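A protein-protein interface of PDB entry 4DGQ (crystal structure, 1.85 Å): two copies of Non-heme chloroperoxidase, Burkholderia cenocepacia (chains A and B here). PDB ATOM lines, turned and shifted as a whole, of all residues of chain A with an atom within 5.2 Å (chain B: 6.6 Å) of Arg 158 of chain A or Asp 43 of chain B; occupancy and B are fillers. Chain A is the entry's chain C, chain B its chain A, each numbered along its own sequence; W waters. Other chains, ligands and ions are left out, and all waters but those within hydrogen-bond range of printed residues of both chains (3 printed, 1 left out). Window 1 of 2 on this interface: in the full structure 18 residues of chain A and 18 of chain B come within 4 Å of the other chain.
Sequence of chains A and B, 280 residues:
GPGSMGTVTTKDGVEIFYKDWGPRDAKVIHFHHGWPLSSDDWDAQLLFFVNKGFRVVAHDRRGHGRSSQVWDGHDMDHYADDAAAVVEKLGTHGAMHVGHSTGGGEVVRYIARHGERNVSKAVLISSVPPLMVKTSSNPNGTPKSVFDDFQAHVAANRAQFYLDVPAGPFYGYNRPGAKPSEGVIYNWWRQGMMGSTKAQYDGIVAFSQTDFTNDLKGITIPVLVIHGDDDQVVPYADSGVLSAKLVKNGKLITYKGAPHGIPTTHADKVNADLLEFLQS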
ATOM      1  N   HIS A 153     -30.512 -24.096   5.283  1.00  0.00           N
ATOM      2  CA  HIS A 153     -30.874 -24.627   6.624  1.00  0.00           C
ATOM      3  C   HIS A 153     -29.678 -24.976   7.444  1.00  0.00           C
ATOM      4  O   HIS A 153     -29.664 -24.713   8.669  1.00  0.00           O
ATOM      5  CB  HIS A 153     -31.811 -25.819   6.518  1.00  0.00           C
ATOM      6  CG  HIS A 153     -33.233 -25.434   6.186  1.00  0.00           C
ATOM      7  ND1 HIS A 153     -34.038 -24.765   7.082  1.00  0.00           N
ATOM      8  CD2 HIS A 153     -34.015 -25.689   5.067  1.00  0.00           C
ATOM      9  CE1 HIS A 153     -35.268 -24.577   6.513  1.00  0.00           C
ATOM     10  NE2 HIS A 153     -35.239 -25.122   5.272  1.00  0.00           N
ATOM     11  N   VAL A 154     -28.679 -25.617   6.832  1.00  0.00           N
ATOM     12  CA  VAL A 154     -27.443 -25.957   7.563  1.00  0.00           C
ATOM     13  C   VAL A 154     -26.792 -24.678   8.061  1.00  0.00           C
ATOM     14  O   VAL A 154     -26.340 -24.596   9.216  1.00  0.00           O
ATOM     15  CB  VAL A 154     -26.462 -26.794   6.717  1.00  0.00           C
ATOM     16  CG1 VAL A 154     -25.092 -26.864   7.366  1.00  0.00           C
ATOM     17  CG2 VAL A 154     -27.028 -28.194   6.475  1.00  0.00           C
ATOM     18  N   ALA A 156     -28.230 -21.707   8.575  1.00  0.00           N
ATOM     19  CA  ALA A 156     -29.121 -20.922   9.470  1.00  0.00           C
ATOM     20  C   ALA A 156     -29.250 -21.516  10.875  1.00  0.00           C
ATOM     21  O   ALA A 156     -29.203 -20.775  11.866  1.00  0.00           O
ATOM     22  CB  ALA A 156     -30.509 -20.784   8.884  1.00  0.00           C
ATOM     23  N   ASN A 157     -29.446 -22.819  10.954  1.00  0.00           N
ATOM     24  CA  ASN A 157     -29.617 -23.502  12.259  1.00  0.00           C
ATOM     25  C   ASN A 157     -29.429 -25.012  12.083  1.00  0.00           C
ATOM     26  O   ASN A 157     -30.380 -25.787  11.977  1.00  0.00           O
ATOM     27  CB  ASN A 157     -30.989 -23.175  12.886  1.00  0.00           C
ATOM     28  CG  ASN A 157     -31.111 -23.662  14.319  1.00  0.00           C
ATOM     29  OD1 ASN A 157     -30.268 -24.436  14.816  1.00  0.00           O
ATOM     30  ND2 ASN A 157     -32.169 -23.192  15.015  1.00  0.00           N
ATOM     31  N   ARG A 158     -28.170 -25.407  12.018  1.00  0.00           N
ATOM     32  CA  ARG A 158     -27.826 -26.794  11.761  1.00  0.00           C
ATOM     33  C   ARG A 158     -28.415 -27.662  12.886  1.00  0.00           C
ATOM     34  O   ARG A 158     -28.908 -28.756  12.619  1.00  0.00           O
ATOM     35  CB  ARG A 158     -26.291 -26.968  11.648  1.00  0.00           C
ATOM     36  CG  ARG A 158     -25.847 -28.398  11.269  1.00  0.00           C
ATOM     37  CD  ARG A 158     -24.330 -28.542  11.097  1.00  0.00           C
ATOM     38  NE  ARG A 158     -23.622 -28.421  12.359  1.00  0.00           N
ATOM     39  CZ  ARG A 158     -22.750 -29.273  12.871  1.00  0.00           C
ATOM     40  NH1 ARG A 158     -22.400 -30.388  12.238  1.00  0.00           N
ATOM     41  NH2 ARG A 158     -22.172 -28.972  14.028  1.00  0.00           N
ATOM     42  N   ALA A 159     -28.329 -27.171  14.126  1.00  0.00           N
ATOM     43  CA  ALA A 159     -28.757 -27.947  15.278  1.00  0.00           C
ATOM     44  C   ALA A 159     -30.234 -28.351  15.173  1.00  0.00           C
ATOM     45  O   ALA A 159     -30.595 -29.461  15.483  1.00  0.00           O
ATOM     46  CB  ALA A 159     -28.469 -27.233  16.594  1.00  0.00           C
ATOM     47  N   GLN A 160     -31.078 -27.425  14.742  1.00  0.00           N
ATOM     48  CA  GLN A 160     -32.502 -27.712  14.560  1.00  0.00           C
ATOM     49  C   GLN A 160     -32.793 -28.520  13.321  1.00  0.00           C
ATOM     50  O   GLN A 160     -33.586 -29.461  13.338  1.00  0.00           O
ATOM     51  CB  GLN A 160     -33.303 -26.404  14.552  1.00  0.00           C
ATOM     52  CG  GLN A 160     -34.827 -26.605  14.593  1.00  0.00           C
ATOM     53  CD  GLN A 160     -35.239 -27.402  15.844  1.00  0.00           C
ATOM     54  OE1 GLN A 160     -34.797 -27.057  16.939  1.00  0.00           O
ATOM     55  NE2 GLN A 160     -36.080 -28.454  15.698  1.00  0.00           N
ATOM     56  N   PHE A 161     -32.163 -28.148  12.210  1.00  0.00           N
ATOM     57  CA  PHE A 161     -32.316 -28.917  10.969  1.00  0.00           C
ATOM     58  C   PHE A 161     -32.020 -30.418  11.165  1.00  0.00           C
ATOM     59  O   PHE A 161     -32.717 -31.261  10.607  1.00  0.00           O
ATOM     60  CB  PHE A 161     -31.425 -28.313   9.867  1.00  0.00           C
ATOM     61  CG  PHE A 161     -31.646 -28.899   8.501  1.00  0.00           C
ATOM     62  CD1 PHE A 161     -32.905 -28.886   7.934  1.00  0.00           C
ATOM     63  CD2 PHE A 161     -30.583 -29.321   7.731  1.00  0.00           C
ATOM     64  CE1 PHE A 161     -33.121 -29.358   6.632  1.00  0.00           C
ATOM     65  CE2 PHE A 161     -30.796 -29.822   6.447  1.00  0.00           C
ATOM     66  CZ  PHE A 161     -32.042 -29.833   5.910  1.00  0.00           C
ATOM     67  N   TYR A 162     -31.027 -30.732  12.010  1.00  0.00           N
ATOM     68  CA  TYR A 162     -30.639 -32.117  12.232  1.00  0.00           C
ATOM     69  C   TYR A 162     -31.573 -32.873  13.183  1.00  0.00           C
ATOM     70  O   TYR A 162     -31.360 -34.054  13.391  1.00  0.00           O
ATOM     71  CB  TYR A 162     -29.164 -32.243  12.634  1.00  0.00           C
ATOM     72  CG  TYR A 162     -28.153 -31.938  11.556  1.00  0.00           C
ATOM     73  CD1 TYR A 162     -26.823 -32.083  11.807  1.00  0.00           C
ATOM     74  CD2 TYR A 162     -28.533 -31.585  10.280  1.00  0.00           C
ATOM     75  CE1 TYR A 162     -25.861 -31.835  10.835  1.00  0.00           C
ATOM     76  CE2 TYR A 162     -27.593 -31.344   9.281  1.00  0.00           C
ATOM     77  CZ  TYR A 162     -26.260 -31.438   9.562  1.00  0.00           C
ATOM     78  OH  TYR A 162     -25.319 -31.146   8.581  1.00  0.00           O
ATOM     79  N   LEU A 163     -32.557 -32.191  13.774  1.00  0.00           N
ATOM     80  CA  LEU A 163     -33.694 -32.862  14.394  1.00  0.00           C
ATOM     81  C   LEU A 163     -34.811 -33.011  13.389  1.00  0.00           C
ATOM     82  O   LEU A 163     -35.482 -34.045  13.331  1.00  0.00           O
ATOM     83  CB  LEU A 163     -34.201 -32.088  15.626  1.00  0.00           C
ATOM     84  CG  LEU A 163     -33.343 -32.136  16.886  1.00  0.00           C
ATOM     85  CD1 LEU A 163     -33.972 -31.300  18.023  1.00  0.00           C
ATOM     86  CD2 LEU A 163     -33.089 -33.588  17.333  1.00  0.00           C
ATOM     87  N   GLY A 192     -24.655 -36.257  13.265  1.00  0.00           N
ATOM     88  CA  GLY A 192     -24.539 -35.069  12.414  1.00  0.00           C
ATOM     89  C   GLY A 192     -23.758 -33.952  13.151  1.00  0.00           C
ATOM     90  O   GLY A 192     -22.815 -33.346  12.604  1.00  0.00           O
ATOM     91  N   MET A 193     -24.115 -33.698  14.409  1.00  0.00           N
ATOM     92  CA  MET A 193     -23.557 -32.574  15.138  1.00  0.00           C
ATOM     93  C   MET A 193     -22.090 -32.705  15.473  1.00  0.00           C
ATOM     94  O   MET A 193     -21.419 -31.668  15.526  1.00  0.00           O
ATOM     95  CB  MET A 193     -24.379 -32.211  16.385  1.00  0.00           C
ATOM     96  CG  MET A 193     -25.789 -31.734  16.074  1.00  0.00           C
ATOM     97  SD  MET A 193     -25.943 -30.390  14.871  1.00  0.00           S
ATOM     98  CE  MET A 193     -25.319 -29.039  15.902  1.00  0.00           C
ATOM     99  N   MET A 194     -21.571 -33.925  15.630  1.00  0.00           N
ATOM    100  CA  MET A 194     -20.126 -34.053  15.879  1.00  0.00           C
ATOM    101  C   MET A 194     -19.242 -33.766  14.668  1.00  0.00           C
ATOM    102  O   MET A 194     -18.047 -33.503  14.815  1.00  0.00           O
ATOM    103  CB  MET A 194     -19.797 -35.418  16.505  1.00  0.00           C
ATOM    104  CG  MET A 194     -19.905 -36.566  15.614  1.00  0.00           C
ATOM    105  SD  MET A 194     -19.236 -38.084  16.440  1.00  0.00           S
ATOM    106  CE  MET A 194     -20.541 -38.303  17.643  1.00  0.00           C
ATOM    107  N   GLY A 195     -19.846 -33.845  13.471  1.00  0.00           N
ATOM    108  CA  GLY A 195     -19.177 -33.503  12.233  1.00  0.00           C
ATOM    109  C   GLY A 195     -19.073 -32.009  12.028  1.00  0.00           C
ATOM    110  O   GLY A 195     -19.605 -31.184  12.819  1.00  0.00           O
ATOM    111  N   SER A 196     -18.333 -31.663  10.989  1.00  0.00           N
ATOM    112  CA  SER A 196     -18.088 -30.258  10.594  1.00  0.00           C
ATOM    113  C   SER A 196     -19.244 -29.656   9.784  1.00  0.00           C
ATOM    114  O   SER A 196     -19.669 -30.244   8.791  1.00  0.00           O
ATOM    115  CB  SER A 196     -16.841 -30.181   9.722  1.00  0.00           C
ATOM    116  OG  SER A 196     -16.811 -28.989   8.916  1.00  0.00           O
ATOM    117  N   THR A 197     -19.729 -28.481  10.222  1.00  0.00           N
ATOM    118  CA  THR A 197     -20.744 -27.773   9.481  1.00  0.00           C
ATOM    119  C   THR A 197     -20.279 -27.460   8.058  1.00  0.00           C
ATOM    120  O   THR A 197     -21.072 -27.549   7.139  1.00  0.00           O
ATOM    121  CB  THR A 197     -21.225 -26.509  10.236  1.00  0.00           C
ATOM    122  OG1 THR A 197     -22.326 -25.946   9.509  1.00  0.00           O
ATOM    123  CG2 THR A 197     -20.123 -25.478  10.281  1.00  0.00           C
ATOM    124  N   GLN A 200     -20.251 -30.682   5.894  1.00  0.00           N
ATOM    125  CA  GLN A 200     -21.633 -31.121   5.609  1.00  0.00           C
ATOM    126  C   GLN A 200     -22.299 -30.160   4.641  1.00  0.00           C
ATOM    127  O   GLN A 200     -23.056 -30.617   3.783  1.00  0.00           O
ATOM    128  CB  GLN A 200     -22.415 -31.300   6.907  1.00  0.00           C
ATOM    129  CG  GLN A 200     -21.777 -32.436   7.749  1.00  0.00           C
ATOM    130  CD  GLN A 200     -22.251 -32.439   9.193  1.00  0.00           C
ATOM    131  OE1 GLN A 200     -22.912 -31.488   9.665  1.00  0.00           O
ATOM    132  NE2 GLN A 200     -21.867 -33.474   9.924  1.00  0.00           N
ATOM    133  N   LYS B  19     -10.331 -25.869  15.154  1.00  0.00           N
ATOM    134  CA  LYS B  19     -10.704 -25.846  13.765  1.00  0.00           C
ATOM    135  C   LYS B  19      -9.880 -24.748  13.074  1.00  0.00           C
ATOM    136  O   LYS B  19      -9.697 -23.664  13.639  1.00  0.00           O
ATOM    137  CB  LYS B  19     -12.215 -25.497  13.683  1.00  0.00           C
ATOM    138  CG  LYS B  19     -13.124 -26.449  14.456  1.00  0.00           C
ATOM    139  CD  LYS B  19     -14.604 -26.058  14.378  1.00  0.00           C
ATOM    140  CE  LYS B  19     -15.520 -26.950  15.240  1.00  0.00           C
ATOM    141  NZ  LYS B  19     -16.828 -27.295  14.598  1.00  0.00           N
ATOM    142  N   TRP B  21      -9.985 -23.357   9.190  1.00  0.00           N
ATOM    143  CA  TRP B  21     -10.649 -23.496   7.899  1.00  0.00           C
ATOM    144  C   TRP B  21     -10.346 -22.303   7.016  1.00  0.00           C
ATOM    145  O   TRP B  21     -10.413 -21.135   7.471  1.00  0.00           O
ATOM    146  CB  TRP B  21     -12.151 -23.566   8.093  1.00  0.00           C
ATOM    147  CG  TRP B  21     -12.671 -24.708   8.918  1.00  0.00           C
ATOM    148  CD1 TRP B  21     -12.007 -25.870   9.303  1.00  0.00           C
ATOM    149  CD2 TRP B  21     -14.013 -24.853   9.397  1.00  0.00           C
ATOM    150  NE1 TRP B  21     -12.848 -26.687  10.010  1.00  0.00           N
ATOM    151  CE2 TRP B  21     -14.078 -26.128  10.080  1.00  0.00           C
ATOM    152  CE3 TRP B  21     -15.171 -24.055   9.336  1.00  0.00           C
ATOM    153  CZ2 TRP B  21     -15.250 -26.576  10.692  1.00  0.00           C
ATOM    154  CZ3 TRP B  21     -16.331 -24.518   9.951  1.00  0.00           C
ATOM    155  CH2 TRP B  21     -16.369 -25.763  10.598  1.00  0.00           C
ATOM    156  N   SER B  39     -15.666 -24.766  20.513  1.00  0.00           N
ATOM    157  CA  SER B  39     -15.564 -24.022  19.249  1.00  0.00           C
ATOM    158  C   SER B  39     -16.786 -24.273  18.352  1.00  0.00           C
ATOM    159  O   SER B  39     -17.063 -23.472  17.448  1.00  0.00           O
ATOM    160  CB  SER B  39     -14.271 -24.348  18.476  1.00  0.00           C
ATOM    161  OG  SER B  39     -14.213 -25.733  18.223  1.00  0.00           O
ATOM    162  N   ASP B  40     -17.550 -25.346  18.606  1.00  0.00           N
ATOM    163  CA  ASP B  40     -18.785 -25.572  17.881  1.00  0.00           C
ATOM    164  C   ASP B  40     -19.810 -24.448  18.074  1.00  0.00           C
ATOM    165  O   ASP B  40     -20.724 -24.267  17.205  1.00  0.00           O
ATOM    166  CB  ASP B  40     -19.428 -26.912  18.302  1.00  0.00           C
ATOM    167  CG  ASP B  40     -18.799 -28.105  17.622  1.00  0.00           C
ATOM    168  OD1 ASP B  40     -17.632 -28.040  17.198  1.00  0.00           O
ATOM    169  OD2 ASP B  40     -19.485 -29.179  17.483  1.00  0.00           O
ATOM    170  N   ASP B  41     -19.694 -23.685  19.168  1.00  0.00           N
ATOM    171  CA  ASP B  41     -20.620 -22.600  19.400  1.00  0.00           C
ATOM    172  C   ASP B  41     -20.475 -21.484  18.344  1.00  0.00           C
ATOM    173  O   ASP B  41     -21.334 -20.604  18.235  1.00  0.00           O
ATOM    174  CB  ASP B  41     -20.468 -22.050  20.813  1.00  0.00           C
ATOM    175  CG  ASP B  41     -21.656 -21.158  21.228  1.00  0.00           C
ATOM    176  OD1 ASP B  41     -22.809 -21.579  20.991  1.00  0.00           O
ATOM    177  OD2 ASP B  41     -21.442 -20.030  21.734  1.00  0.00           O
ATOM    178  N   TRP B  42     -19.384 -21.507  17.557  1.00  0.00           N
ATOM    179  CA  TRP B  42     -19.166 -20.502  16.529  1.00  0.00           C
ATOM    180  C   TRP B  42     -19.541 -20.936  15.148  1.00  0.00           C
ATOM    181  O   TRP B  42     -19.269 -20.205  14.161  1.00  0.00           O
ATOM    182  CB  TRP B  42     -17.722 -20.168  16.486  1.00  0.00           C
ATOM    183  CG  TRP B  42     -17.229 -19.428  17.649  1.00  0.00           C
ATOM    184  CD1 TRP B  42     -16.309 -19.839  18.620  1.00  0.00           C
ATOM    185  CD2 TRP B  42     -17.593 -18.086  18.000  1.00  0.00           C
ATOM    186  NE1 TRP B  42     -16.101 -18.839  19.519  1.00  0.00           N
ATOM    187  CE2 TRP B  42     -16.796 -17.737  19.154  1.00  0.00           C
ATOM    188  CE3 TRP B  42     -18.421 -17.119  17.421  1.00  0.00           C
ATOM    189  CZ2 TRP B  42     -16.893 -16.495  19.733  1.00  0.00           C
ATOM    190  CZ3 TRP B  42     -18.489 -15.859  18.018  1.00  0.00           C
ATOM    191  CH2 TRP B  42     -17.712 -15.553  19.132  1.00  0.00           C
ATOM    192  N   ASP B  43     -20.174 -22.098  15.033  1.00  0.00           N
ATOM    193  CA  ASP B  43     -20.419 -22.677  13.711  1.00  0.00           C
ATOM    194  C   ASP B  43     -21.035 -21.707  12.694  1.00  0.00           C
ATOM    195  O   ASP B  43     -20.645 -21.709  11.521  1.00  0.00           O
ATOM    196  CB  ASP B  43     -21.320 -23.903  13.805  1.00  0.00           C
ATOM    197  CG  ASP B  43     -20.526 -25.193  14.157  1.00  0.00           C
ATOM    198  OD1 ASP B  43     -19.240 -25.178  14.189  1.00  0.00           O
ATOM    199  OD2 ASP B  43     -21.206 -26.167  14.472  1.00  0.00           O
ATOM    200  N   ALA B  44     -22.050 -20.954  13.123  1.00  0.00           N
ATOM    201  CA  ALA B  44     -22.728 -19.997  12.225  1.00  0.00           C
ATOM    202  C   ALA B  44     -21.728 -18.954  11.654  1.00  0.00           C
ATOM    203  O   ALA B  44     -21.784 -18.607  10.432  1.00  0.00           O
ATOM    204  CB  ALA B  44     -23.906 -19.274  12.938  1.00  0.00           C
ATOM    205  N   GLN B  45     -20.824 -18.471  12.509  1.00  0.00           N
ATOM    206  CA  GLN B  45     -19.820 -17.518  12.103  1.00  0.00           C
ATOM    207  C   GLN B  45     -18.712 -18.143  11.252  1.00  0.00           C
ATOM    208  O   GLN B  45     -18.290 -17.567  10.274  1.00  0.00           O
ATOM    209  CB  GLN B  45     -19.205 -16.797  13.302  1.00  0.00           C
ATOM    210  CG  GLN B  45     -20.103 -15.747  13.956  1.00  0.00           C
ATOM    211  CD  GLN B  45     -21.336 -16.355  14.609  1.00  0.00           C
ATOM    212  OE1 GLN B  45     -21.213 -17.319  15.362  1.00  0.00           O
ATOM    213  NE2 GLN B  45     -22.520 -15.854  14.254  1.00  0.00           N
ATOM    214  N   LEU B  46     -18.220 -19.292  11.650  1.00  0.00           N
ATOM    215  CA  LEU B  46     -17.148 -19.963  10.938  1.00  0.00           C
ATOM    216  C   LEU B  46     -17.557 -20.256   9.494  1.00  0.00           C
ATOM    217  O   LEU B  46     -16.797 -19.992   8.562  1.00  0.00           O
ATOM    218  CB  LEU B  46     -16.757 -21.250  11.631  1.00  0.00           C
ATOM    219  CG  LEU B  46     -16.278 -21.186  13.076  1.00  0.00           C
ATOM    220  CD1 LEU B  46     -15.828 -22.583  13.527  1.00  0.00           C
ATOM    221  CD2 LEU B  46     -15.173 -20.171  13.257  1.00  0.00           C
ATOM    222  N   LEU B  47     -18.763 -20.781   9.322  1.00  0.00           N
ATOM    223  CA  LEU B  47     -19.308 -21.064   8.003  1.00  0.00           C
ATOM    224  C   LEU B  47     -19.456 -19.801   7.155  1.00  0.00           C
ATOM    225  O   LEU B  47     -19.054 -19.793   6.007  1.00  0.00           O
ATOM    226  CB  LEU B  47     -20.618 -21.823   8.082  1.00  0.00           C
ATOM    227  CG  LEU B  47     -21.182 -22.398   6.768  1.00  0.00           C
ATOM    228  CD1 LEU B  47     -20.206 -23.371   6.094  1.00  0.00           C
ATOM    229  CD2 LEU B  47     -22.537 -23.098   7.040  1.00  0.00           C
ATOM    230  N   PHE B  48     -20.005 -18.738   7.733  1.00  0.00           N
ATOM    231  CA  PHE B  48     -20.175 -17.487   7.036  1.00  0.00           C
ATOM    232  C   PHE B  48     -18.842 -16.989   6.505  1.00  0.00           C
ATOM    233  O   PHE B  48     -18.740 -16.613   5.327  1.00  0.00           O
ATOM    234  CB  PHE B  48     -20.793 -16.467   7.969  1.00  0.00           C
ATOM    235  CG  PHE B  48     -20.865 -15.090   7.409  1.00  0.00           C
ATOM    236  CD1 PHE B  48     -19.889 -14.158   7.694  1.00  0.00           C
ATOM    237  CD2 PHE B  48     -21.971 -14.707   6.678  1.00  0.00           C
ATOM    238  CE1 PHE B  48     -20.014 -12.848   7.230  1.00  0.00           C
ATOM    239  CE2 PHE B  48     -22.080 -13.439   6.173  1.00  0.00           C
ATOM    240  CZ  PHE B  48     -21.092 -12.492   6.478  1.00  0.00           C
ATOM    241  N   ASN B 187     -27.856 -28.868  21.656  1.00  0.00           N
ATOM    242  CA  ASN B 187     -26.480 -28.657  21.174  1.00  0.00           C
ATOM    243  C   ASN B 187     -25.609 -27.987  22.249  1.00  0.00           C
ATOM    244  O   ASN B 187     -24.429 -28.333  22.418  1.00  0.00           O
ATOM    245  CB  ASN B 187     -26.472 -27.834  19.889  1.00  0.00           C
ATOM    246  CG  ASN B 187     -25.136 -27.902  19.166  1.00  0.00           C
ATOM    247  OD1 ASN B 187     -24.463 -28.942  19.196  1.00  0.00           O
ATOM    248  ND2 ASN B 187     -24.771 -26.810  18.486  1.00  0.00           N
ATOM    249  N   ARG B 190     -24.923 -30.709  24.777  1.00  0.00           N
ATOM    250  CA  ARG B 190     -23.973 -31.686  24.214  1.00  0.00           C
ATOM    251  C   ARG B 190     -22.548 -31.193  24.355  1.00  0.00           C
ATOM    252  O   ARG B 190     -21.691 -31.901  24.789  1.00  0.00           O
ATOM    253  CB  ARG B 190     -24.294 -31.899  22.716  1.00  0.00           C
ATOM    254  CG  ARG B 190     -23.397 -32.841  21.894  1.00  0.00           C
ATOM    255  CD  ARG B 190     -23.742 -32.804  20.386  1.00  0.00           C
ATOM    256  NE  ARG B 190     -23.363 -31.546  19.795  1.00  0.00           N
ATOM    257  CZ  ARG B 190     -22.165 -31.296  19.298  1.00  0.00           C
ATOM    258  NH1 ARG B 190     -21.250 -32.260  19.282  1.00  0.00           N
ATOM    259  NH2 ARG B 190     -21.876 -30.098  18.808  1.00  0.00           N
HETATM  260  O   HOH W   1     -14.475 -28.544   8.023  1.00  0.00           O
HETATM  261  O   HOH W   2     -18.972 -27.826  12.908  1.00  0.00           O
HETATM  262  O   HOH W   3     -22.324 -27.185  16.521  1.00  0.00           O
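The guanidinium group (NH2) of Arg 158 of chain A lies within salt-bridge range of the side-chain carboxylate (OD2) of Asp 43 of chain B (3.0 Å).
The side-chain amino group (NZ) of Lys 19 of chain B is in salt-bridge range of the side-chain carboxylate (OD1) of Asp 40 of chain B, at 2.8 Å.
The side-chain carboxylate (OD2) of Asp 40 of chain B lies within salt-bridge range of the guanidinium group (NH2) of Arg 190 of chain B (2.9 Å).
The side-chain amide oxygen (OD1) of Asn 157 of chain A sits close to the backbone NH (N) of Ala 159 of chain A (3.4 Å).
NH1 of Arg 158 of chain A lies within hydrogen-bond range of O of Gly 192 of chain A (3.0 Å).
The guanidinium group of Arg 158 of chain A lies within hydrogen-bond range of the backbone carbonyl oxygen of Met 193 of chain A.
The guanidinium group of Arg 158 of chain A lies within hydrogen-bond range of the side-chain amide oxygen of Gln 200 of chain A, at 2.8 Å.
Among the printed residues, pairs that only touch across the chains: Ala 159 of chain A with Asn 187 of chain B, Met 193 of chain A with Asp 40 of chain B, Met 193 of chain A with Asn 187 of chain B, Met 193 of chain A with Arg 190 of chain B, Ser 196 of chain A with Trp 21 of chain B, Thr 197 of chain A with Trp 21 of chain B, Thr 197 of chain A with Asp 43 of chain B and Thr 197 of chain A with Leu 47 of chain B.
Arg 158 of chain A touches one residue of chain B.
Printed residues of chain B within 4 Å of Met 193 of chain A: Asp 40 (3.7 Å), Asn 187 (3.4 Å) and Arg 190 (3.6 Å).
Printed residues of chain B within 4 Å of Ser 196 of chain A: Trp 21.
Of chain A, only Arg 158 (3.0 Å) and Thr 197 (3.9 Å) come within 4 Å of Asp 43 of chain B.
Printed residues of chain A within 4 Å of Arg 190 of chain B: Met 193 (3.6 Å).
The nearest printed residue of chain A that does not touch Asp 43 of chain B is Met 193 of chain A (5.2 Å).
The nearest printed residue of chain B that does not touch Ala 159 of chain A is Asp 43 of chain B (7.2 Å).
Of the 14 printed residues of chain B, 6 touch a printed residue of chain A.
Printed residues of chain B that touch a printed residue of chain A: Trp 21, Asp 40, Asp 43, Leu 47, Asn 187 and Arg 190.
Along chain B the printed residues that touch a printed residue of chain A span positions 21 to 190.
Hydrophobic or aromatic side chains of chain A within 4 Å of the printed part of chain B: Ala 159 and Met 193.
Among the printed residues, 9 pairs touch across the chains.
Among the printed residues, Asp or Glu carboxylates within 4 Å of a Lys or Arg side-chain nitrogen of the other chain: Arg 158 of chain A with Asp 43 of chain B.
No position is printed for both chains.
Water W1 lies within hydrogen-bond range of the side-chain hydroxyl (OG) of Ser 196 of chain A (2.5 Å) and the indole nitrogen (NE1) of Trp 21 of chain B (3.2 Å).
Water W3 lies within hydrogen-bond range of the side-chain carboxylate of Asp 43 of chain B (2.5 Å), the guanidinium group of Arg 158 of chain A (3.1 Å), the side-chain amide nitrogen of Asn 187 of chain B (3.2 Å) and the backbone carbonyl oxygen of Asp 40 of chain B (3.4 Å).
Water W2 lies within hydrogen-bond range of the side-chain amino group (NZ) of Lys 19 of chain B (2.8 Å), the backbone NH (N) of Thr 197 of chain A (2.9 Å), the side-chain carboxylate (OD1) of Asp 43 of chain B (3.0 Å) and the backbone carbonyl oxygen (O) of Gly 195 of chain A (3.4 Å).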
